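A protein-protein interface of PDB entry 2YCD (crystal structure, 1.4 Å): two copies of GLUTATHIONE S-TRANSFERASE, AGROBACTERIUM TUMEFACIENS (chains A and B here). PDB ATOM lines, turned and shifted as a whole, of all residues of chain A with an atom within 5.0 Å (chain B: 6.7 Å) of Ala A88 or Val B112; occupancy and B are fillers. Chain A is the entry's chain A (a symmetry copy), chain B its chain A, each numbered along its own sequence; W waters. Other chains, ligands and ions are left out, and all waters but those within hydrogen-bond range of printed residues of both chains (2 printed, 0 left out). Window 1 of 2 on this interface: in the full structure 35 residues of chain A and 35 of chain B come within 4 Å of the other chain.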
ATOM      1  N   LEU A  83     -10.829  21.269  16.471  1.00  0.00           N
ATOM      2  CA  LEU A  83     -10.880  22.012  17.730  1.00  0.00           C
ATOM      3  C   LEU A  83     -10.006  21.346  18.752  1.00  0.00           C
ATOM      4  O   LEU A  83      -9.743  20.124  18.692  1.00  0.00           O
ATOM      5  CB  LEU A  83     -12.294  22.055  18.314  1.00  0.00           C
ATOM      6  CG  LEU A  83     -13.378  22.770  17.541  1.00  0.00           C
ATOM      7  CD1 LEU A  83     -14.704  22.575  18.275  1.00  0.00           C
ATOM      8  CD2 LEU A  83     -13.032  24.244  17.481  1.00  0.00           C
ATOM      9  N   PHE A  84      -9.578  22.138  19.729  1.00  0.00           N
ATOM     10  CA  PHE A  84      -8.956  21.607  20.930  1.00  0.00           C
ATOM     11  C   PHE A  84      -9.531  22.370  22.126  1.00  0.00           C
ATOM     12  O   PHE A  84     -10.347  23.285  21.936  1.00  0.00           O
ATOM     13  CB  PHE A  84      -7.420  21.620  20.836  1.00  0.00           C
ATOM     14  CG  PHE A  84      -6.806  22.973  20.969  1.00  0.00           C
ATOM     15  CD1 PHE A  84      -6.856  23.866  19.917  1.00  0.00           C
ATOM     16  CD2 PHE A  84      -6.176  23.353  22.140  1.00  0.00           C
ATOM     17  CE1 PHE A  84      -6.265  25.138  20.022  1.00  0.00           C
ATOM     18  CE2 PHE A  84      -5.592  24.616  22.267  1.00  0.00           C
ATOM     19  CZ  PHE A  84      -5.654  25.514  21.209  1.00  0.00           C
ATOM     20  N   GLU A  85      -9.103  21.970  23.321  1.00  0.00           N
ATOM     21  CA  GLU A  85      -9.633  22.432  24.624  1.00  0.00           C
ATOM     22  C   GLU A  85     -10.928  21.732  24.966  1.00  0.00           C
ATOM     23  O   GLU A  85     -11.953  22.000  24.353  1.00  0.00           O
ATOM     24  CB  GLU A  85      -9.806  23.953  24.716  1.00  0.00           C
ATOM     25  CG  GLU A  85      -8.466  24.718  24.701  1.00  0.00           C
ATOM     26  CD  GLU A  85      -7.588  24.412  25.890  1.00  0.00           C
ATOM     27  OE1 GLU A  85      -8.105  24.121  26.992  1.00  0.00           O
ATOM     28  OE2 GLU A  85      -6.352  24.480  25.733  1.00  0.00           O
ATOM     29  N   SER A  86     -10.871  20.816  25.930  1.00  0.00           N
ATOM     30  CA  SER A  86     -12.065  20.112  26.382  1.00  0.00           C
ATOM     31  C   SER A  86     -13.243  21.047  26.670  1.00  0.00           C
ATOM     32  O   SER A  86     -14.373  20.742  26.281  1.00  0.00           O
ATOM     33  CB  SER A  86     -11.730  19.228  27.594  1.00  0.00           C
ATOM     34  OG  SER A  86     -11.316  20.011  28.696  1.00  0.00           O
ATOM     35  N   GLY A  87     -12.979  22.202  27.294  1.00  0.00           N
ATOM     36  CA  GLY A  87     -14.059  23.143  27.575  1.00  0.00           C
ATOM     37  C   GLY A  87     -14.703  23.694  26.300  1.00  0.00           C
ATOM     38  O   GLY A  87     -15.927  23.857  26.216  1.00  0.00           O
ATOM     39  N   ALA A  88     -13.875  24.012  25.300  1.00  0.00           N
ATOM     40  CA  ALA A  88     -14.354  24.572  24.043  1.00  0.00           C
ATOM     41  C   ALA A  88     -15.032  23.526  23.162  1.00  0.00           C
ATOM     42  O   ALA A  88     -15.933  23.839  22.374  1.00  0.00           O
ATOM     43  CB  ALA A  88     -13.203  25.204  23.284  1.00  0.00           C
ATOM     44  N   ILE A  89     -14.585  22.280  23.277  1.00  0.00           N
ATOM     45  CA  ILE A  89     -15.189  21.172  22.540  1.00  0.00           C
ATOM     46  C   ILE A  89     -16.590  20.902  23.095  1.00  0.00           C
ATOM     47  O   ILE A  89     -17.567  20.807  22.341  1.00  0.00           O
ATOM     48  CB  ILE A  89     -14.282  19.918  22.588  1.00  0.00           C
ATOM     49  CG1 ILE A  89     -12.963  20.174  21.837  1.00  0.00           C
ATOM     50  CG2 ILE A  89     -15.018  18.715  21.954  1.00  0.00           C
ATOM     51  CD1 ILE A  89     -11.883  19.133  22.165  1.00  0.00           C
ATOM     52  N   VAL A  90     -16.701  20.820  24.417  1.00  0.00           N
ATOM     53  CA  VAL A  90     -18.008  20.732  25.058  1.00  0.00           C
ATOM     54  C   VAL A  90     -18.895  21.916  24.685  1.00  0.00           C
ATOM     55  O   VAL A  90     -20.059  21.713  24.320  1.00  0.00           O
ATOM     56  CB  VAL A  90     -17.866  20.557  26.575  1.00  0.00           C
ATOM     57  CG1 VAL A  90     -19.210  20.705  27.275  1.00  0.00           C
ATOM     58  CG2 VAL A  90     -17.234  19.184  26.890  1.00  0.00           C
ATOM     59  N   MET A  91     -18.340  23.130  24.668  1.00  0.00           N
ATOM     60  CA  MET A  91     -19.115  24.302  24.256  1.00  0.00           C
ATOM     61  C   MET A  91     -19.687  24.138  22.850  1.00  0.00           C
ATOM     62  O   MET A  91     -20.867  24.387  22.607  1.00  0.00           O
ATOM     63  CB  MET A  91     -18.247  25.563  24.320  1.00  0.00           C
ATOM     64  CG  MET A  91     -19.029  26.837  24.053  1.00  0.00           C
ATOM     65  SD  MET A  91     -20.155  27.245  25.396  1.00  0.00           S
ATOM     66  CE  MET A  91     -19.041  28.106  26.497  1.00  0.00           C
ATOM     67  N   HIS A  92     -18.840  23.726  21.914  1.00  0.00           N
ATOM     68  CA  HIS A  92     -19.261  23.544  20.525  1.00  0.00           C
ATOM     69  C   HIS A  92     -20.376  22.520  20.375  1.00  0.00           C
ATOM     70  O   HIS A  92     -21.366  22.762  19.660  1.00  0.00           O
ATOM     71  CB  HIS A  92     -18.057  23.165  19.650  1.00  0.00           C
ATOM     72  CG  HIS A  92     -18.404  22.896  18.216  1.00  0.00           C
ATOM     73  ND1 HIS A  92     -18.741  23.898  17.334  1.00  0.00           N
ATOM     74  CD2 HIS A  92     -18.471  21.737  17.520  1.00  0.00           C
ATOM     75  CE1 HIS A  92     -18.981  23.370  16.145  1.00  0.00           C
ATOM     76  NE2 HIS A  92     -18.837  22.062  16.233  1.00  0.00           N
ATOM     77  N   MET B  91     -16.936  36.449  27.164  1.00  0.00           N
ATOM     78  CA  MET B  91     -17.767  35.701  26.220  1.00  0.00           C
ATOM     79  C   MET B  91     -19.121  36.373  25.999  1.00  0.00           C
ATOM     80  O   MET B  91     -19.568  36.553  24.868  1.00  0.00           O
ATOM     81  CB  MET B  91     -17.974  34.265  26.713  1.00  0.00           C
ATOM     82  CG  MET B  91     -18.699  33.389  25.708  1.00  0.00           C
ATOM     83  SD  MET B  91     -17.684  33.010  24.271  1.00  0.00           S
ATOM     84  CE  MET B  91     -16.761  31.612  24.891  1.00  0.00           C
ATOM     85  N   GLN B  95     -20.633  37.928  22.582  1.00  0.00           N
ATOM     86  CA  GLN B  95     -21.764  37.258  21.934  1.00  0.00           C
ATOM     87  C   GLN B  95     -22.868  38.247  21.560  1.00  0.00           C
ATOM     88  O   GLN B  95     -23.673  37.973  20.667  1.00  0.00           O
ATOM     89  CB  GLN B  95     -22.337  36.147  22.834  1.00  0.00           C
ATOM     90  CG  GLN B  95     -21.423  34.934  23.062  1.00  0.00           C
ATOM     91  CD  GLN B  95     -21.423  33.932  21.911  1.00  0.00           C
ATOM     92  OE1 GLN B  95     -22.153  34.086  20.936  1.00  0.00           O
ATOM     93  NE2 GLN B  95     -20.593  32.895  22.027  1.00  0.00           N
ATOM     94  N   LEU B 101     -16.098  38.323  18.074  1.00  0.00           N
ATOM     95  CA  LEU B 101     -16.253  36.944  17.611  1.00  0.00           C
ATOM     96  C   LEU B 101     -16.632  36.982  16.138  1.00  0.00           C
ATOM     97  O   LEU B 101     -17.448  37.806  15.732  1.00  0.00           O
ATOM     98  CB  LEU B 101     -17.326  36.216  18.425  1.00  0.00           C
ATOM     99  CG  LEU B 101     -16.979  35.744  19.839  1.00  0.00           C
ATOM    100  CD1 LEU B 101     -18.196  35.125  20.517  1.00  0.00           C
ATOM    101  CD2 LEU B 101     -15.803  34.754  19.843  1.00  0.00           C
ATOM    102  N   ARG B 107     -14.941  29.520  12.205  1.00  0.00           N
ATOM    103  CA  ARG B 107     -13.997  30.471  12.781  1.00  0.00           C
ATOM    104  C   ARG B 107     -14.381  30.815  14.217  1.00  0.00           C
ATOM    105  O   ARG B 107     -13.515  30.958  15.087  1.00  0.00           O
ATOM    106  CB  ARG B 107     -13.927  31.735  11.918  1.00  0.00           C
ATOM    107  CG  ARG B 107     -13.387  31.470  10.517  1.00  0.00           C
ATOM    108  CD  ARG B 107     -13.369  32.733   9.668  1.00  0.00           C
ATOM    109  NE  ARG B 107     -14.567  33.545   9.868  1.00  0.00           N
ATOM    110  CZ  ARG B 107     -14.917  34.567   9.095  1.00  0.00           C
ATOM    111  NH1 ARG B 107     -14.166  34.898   8.052  1.00  0.00           N
ATOM    112  NH2 ARG B 107     -16.022  35.255   9.361  1.00  0.00           N
ATOM    113  N   ARG B 108     -15.669  30.940  14.479  1.00  0.00           N
ATOM    114  CA  ARG B 108     -16.151  31.232  15.816  1.00  0.00           C
ATOM    115  C   ARG B 108     -15.775  30.125  16.810  1.00  0.00           C
ATOM    116  O   ARG B 108     -15.316  30.400  17.921  1.00  0.00           O
ATOM    117  CB  ARG B 108     -17.663  31.415  15.784  1.00  0.00           C
ATOM    118  CG  ARG B 108     -18.249  32.199  16.936  1.00  0.00           C
ATOM    119  CD  ARG B 108     -19.757  32.283  16.765  1.00  0.00           C
ATOM    120  NE  ARG B 108     -20.415  33.145  17.743  1.00  0.00           N
ATOM    121  CZ  ARG B 108     -20.635  34.444  17.555  1.00  0.00           C
ATOM    122  NH1 ARG B 108     -20.239  35.030  16.433  1.00  0.00           N
ATOM    123  NH2 ARG B 108     -21.255  35.157  18.489  1.00  0.00           N
ATOM    124  N   ALA B 109     -15.969  28.869  16.411  1.00  0.00           N
ATOM    125  CA  ALA B 109     -15.650  27.743  17.275  1.00  0.00           C
ATOM    126  C   ALA B 109     -14.162  27.709  17.597  1.00  0.00           C
ATOM    127  O   ALA B 109     -13.773  27.392  18.732  1.00  0.00           O
ATOM    128  CB  ALA B 109     -16.116  26.431  16.618  1.00  0.00           C
ATOM    129  N   ARG B 110     -13.314  28.013  16.616  1.00  0.00           N
ATOM    130  CA  ARG B 110     -11.881  28.054  16.870  1.00  0.00           C
ATOM    131  C   ARG B 110     -11.486  29.233  17.772  1.00  0.00           C
ATOM    132  O   ARG B 110     -10.552  29.118  18.576  1.00  0.00           O
ATOM    133  CB  ARG B 110     -11.092  28.085  15.559  1.00  0.00           C
ATOM    134  CG  ARG B 110     -11.325  26.827  14.721  1.00  0.00           C
ATOM    135  CD  ARG B 110     -10.215  26.645  13.700  1.00  0.00           C
ATOM    136  NE  ARG B 110     -10.199  27.751  12.747  1.00  0.00           N
ATOM    137  CZ  ARG B 110     -10.865  27.757  11.594  1.00  0.00           C
ATOM    138  NH1 ARG B 110     -11.593  26.706  11.239  1.00  0.00           N
ATOM    139  NH2 ARG B 110     -10.799  28.814  10.789  1.00  0.00           N
ATOM    140  N   THR B 111     -12.191  30.355  17.657  1.00  0.00           N
ATOM    141  CA  THR B 111     -11.942  31.499  18.528  1.00  0.00           C
ATOM    142  C   THR B 111     -12.234  31.097  19.975  1.00  0.00           C
ATOM    143  O   THR B 111     -11.450  31.396  20.889  1.00  0.00           O
ATOM    144  CB  THR B 111     -12.807  32.695  18.106  1.00  0.00           C
ATOM    145  OG1 THR B 111     -12.521  33.017  16.736  1.00  0.00           O
ATOM    146  CG2 THR B 111     -12.486  33.923  18.961  1.00  0.00           C
ATOM    147  N   VAL B 112     -13.347  30.400  20.187  1.00  0.00           N
ATOM    148  CA  VAL B 112     -13.693  29.914  21.520  1.00  0.00           C
ATOM    149  C   VAL B 112     -12.633  28.916  22.026  1.00  0.00           C
ATOM    150  O   VAL B 112     -12.258  28.959  23.210  1.00  0.00           O
ATOM    151  CB  VAL B 112     -15.127  29.307  21.516  1.00  0.00           C
ATOM    152  CG1 VAL B 112     -15.444  28.586  22.822  1.00  0.00           C
ATOM    153  CG2 VAL B 112     -16.158  30.407  21.232  1.00  0.00           C
ATOM    154  N   ALA B 113     -12.124  28.027  21.163  1.00  0.00           N
ATOM    155  CA  ALA B 113     -11.002  27.181  21.564  1.00  0.00           C
ATOM    156  C   ALA B 113      -9.836  28.007  22.152  1.00  0.00           C
ATOM    157  O   ALA B 113      -9.287  27.664  23.207  1.00  0.00           O
ATOM    158  CB  ALA B 113     -10.525  26.296  20.396  1.00  0.00           C
ATOM    159  N   TRP B 114      -9.461  29.092  21.477  1.00  0.00           N
ATOM    160  CA  TRP B 114      -8.340  29.899  21.947  1.00  0.00           C
ATOM    161  C   TRP B 114      -8.665  30.680  23.219  1.00  0.00           C
ATOM    162  O   TRP B 114      -7.770  30.911  24.029  1.00  0.00           O
ATOM    163  CB  TRP B 114      -7.804  30.811  20.819  1.00  0.00           C
ATOM    164  CG  TRP B 114      -6.909  30.029  19.888  1.00  0.00           C
ATOM    165  CD1 TRP B 114      -7.184  29.653  18.610  1.00  0.00           C
ATOM    166  CD2 TRP B 114      -5.624  29.479  20.208  1.00  0.00           C
ATOM    167  NE1 TRP B 114      -6.120  28.924  18.094  1.00  0.00           N
ATOM    168  CE2 TRP B 114      -5.152  28.813  19.061  1.00  0.00           C
ATOM    169  CE3 TRP B 114      -4.803  29.543  21.331  1.00  0.00           C
ATOM    170  CZ2 TRP B 114      -3.906  28.161  19.033  1.00  0.00           C
ATOM    171  CZ3 TRP B 114      -3.568  28.888  21.306  1.00  0.00           C
ATOM    172  CH2 TRP B 114      -3.128  28.229  20.162  1.00  0.00           C
ATOM    173  N   MET B 115      -9.928  31.059  23.421  1.00  0.00           N
ATOM    174  CA  MET B 115     -10.343  31.645  24.712  1.00  0.00           C
ATOM    175  C   MET B 115     -10.093  30.658  25.859  1.00  0.00           C
ATOM    176  O   MET B 115      -9.490  31.010  26.884  1.00  0.00           O
ATOM    177  CB  MET B 115     -11.820  32.071  24.680  1.00  0.00           C
ATOM    178  CG  MET B 115     -12.097  33.224  23.695  1.00  0.00           C
ATOM    179  SD  MET B 115     -13.860  33.568  23.505  1.00  0.00           S
ATOM    180  CE  MET B 115     -14.208  34.304  25.110  1.00  0.00           C
ATOM    181  N   PHE B 116     -10.536  29.420  25.682  1.00  0.00           N
ATOM    182  CA  PHE B 116     -10.258  28.385  26.678  1.00  0.00           C
ATOM    183  C   PHE B 116      -8.774  28.071  26.826  1.00  0.00           C
ATOM    184  O   PHE B 116      -8.295  27.852  27.936  1.00  0.00           O
ATOM    185  CB  PHE B 116     -11.078  27.113  26.420  1.00  0.00           C
ATOM    186  CG  PHE B 116     -12.522  27.207  26.879  1.00  0.00           C
ATOM    187  CD1 PHE B 116     -13.509  27.731  26.046  1.00  0.00           C
ATOM    188  CD2 PHE B 116     -12.888  26.771  28.135  1.00  0.00           C
ATOM    189  CE1 PHE B 116     -14.842  27.803  26.466  1.00  0.00           C
ATOM    190  CE2 PHE B 116     -14.208  26.844  28.574  1.00  0.00           C
ATOM    191  CZ  PHE B 116     -15.192  27.368  27.733  1.00  0.00           C
ATOM    192  N   ALA B 117      -8.029  28.054  25.720  1.00  0.00           N
ATOM    193  CA  ALA B 117      -6.593  27.785  25.800  1.00  0.00           C
ATOM    194  C   ALA B 117      -5.851  28.849  26.601  1.00  0.00           C
ATOM    195  O   ALA B 117      -4.950  28.536  27.379  1.00  0.00           O
ATOM    196  CB  ALA B 117      -5.992  27.670  24.410  1.00  0.00           C
ATOM    197  N   ALA B 177     -10.415  36.055  21.983  1.00  0.00           N
ATOM    198  CA  ALA B 177      -9.311  35.177  22.362  1.00  0.00           C
ATOM    199  C   ALA B 177      -8.036  35.981  22.599  1.00  0.00           C
ATOM    200  O   ALA B 177      -7.255  35.677  23.506  1.00  0.00           O
ATOM    201  CB  ALA B 177      -9.072  34.085  21.296  1.00  0.00           C
HETATM  202  O   HOH W   1     -15.917  25.966  20.345  1.00  0.00           O
HETATM  203  O   HOH W   2     -19.769  30.352  24.117  1.00  0.00           O
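Leu A83 touches Arg B110 (CD2 to N, 3.9 Å).
Phe A84 touches Ala B113.
CZ of Phe A84 touches CZ2 of Trp B114 (3.8 Å).
CE2 of Phe A84 touches CB of Ala B117, at 3.8 Å.
Ala B113 touches Glu A85 (O to CG, 3.4 Å).
Glu A85 touches Phe B116 (CB to CB, 3.8 Å).
OE2 of Glu A85 touches CA of Ala B117, 3.3 Å away.
CE2 of Phe B116 touches CA of Gly A87, 3.8 Å away.
Ala A88 touches Phe B116 (CB to CD1, 3.8 Å).
His A92 touches Ala B109.
Of the printed residues of chain B, Ala A88 touches Val B112 (3.9 Å), Ala B113 (3.4 Å) and Phe B116 (3.8 Å).
Printed residues of chain A within 4 Å of Val B112: Ala A88 (3.9 Å).
Of the printed residues of chain B, Gly A87 touches Phe B116 (3.8 Å).
Of the printed residues of chain A, Trp B114 touches Phe A84.
Leu B101 touches none of the printed residues of chain A.
Ala B177 touches none of the printed residues of chain A.
The nearest printed residue of chain A that does not touch Val B112 is Met A91 (4.2 Å).
Of the 15 printed residues of chain B, 7 touch a printed residue of chain A.
Hydrophobic or aromatic side chains of chain B that line the printed part of chain A: Ala B109, Ala B113, Trp B114, Phe B116 and Ala B117.
Among the printed residues, 13 pairs touch across the chains.
Among the printed residues, no Asp or Glu carboxylate lies within 4 Å of a Lys or Arg side-chain nitrogen of the other chain.
Water W1 bridges O of Ala A88 (2.9 Å) and O of Ala B109 (3.0 Å).
Water W2 lies within hydrogen-bond range of the side-chain sulfur (SD) of Met B91 (3.4 Å), the side-chain sulfur (SD) of Met A91 (3.4 Å) and the side-chain amide nitrogen (NE2) of Gln B95 (3.4 Å).
Position printed for both chains: 91.
Of the 13 pairs that touch across the chains among the printed residues, none has its exchanged pair printed and touching as well.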
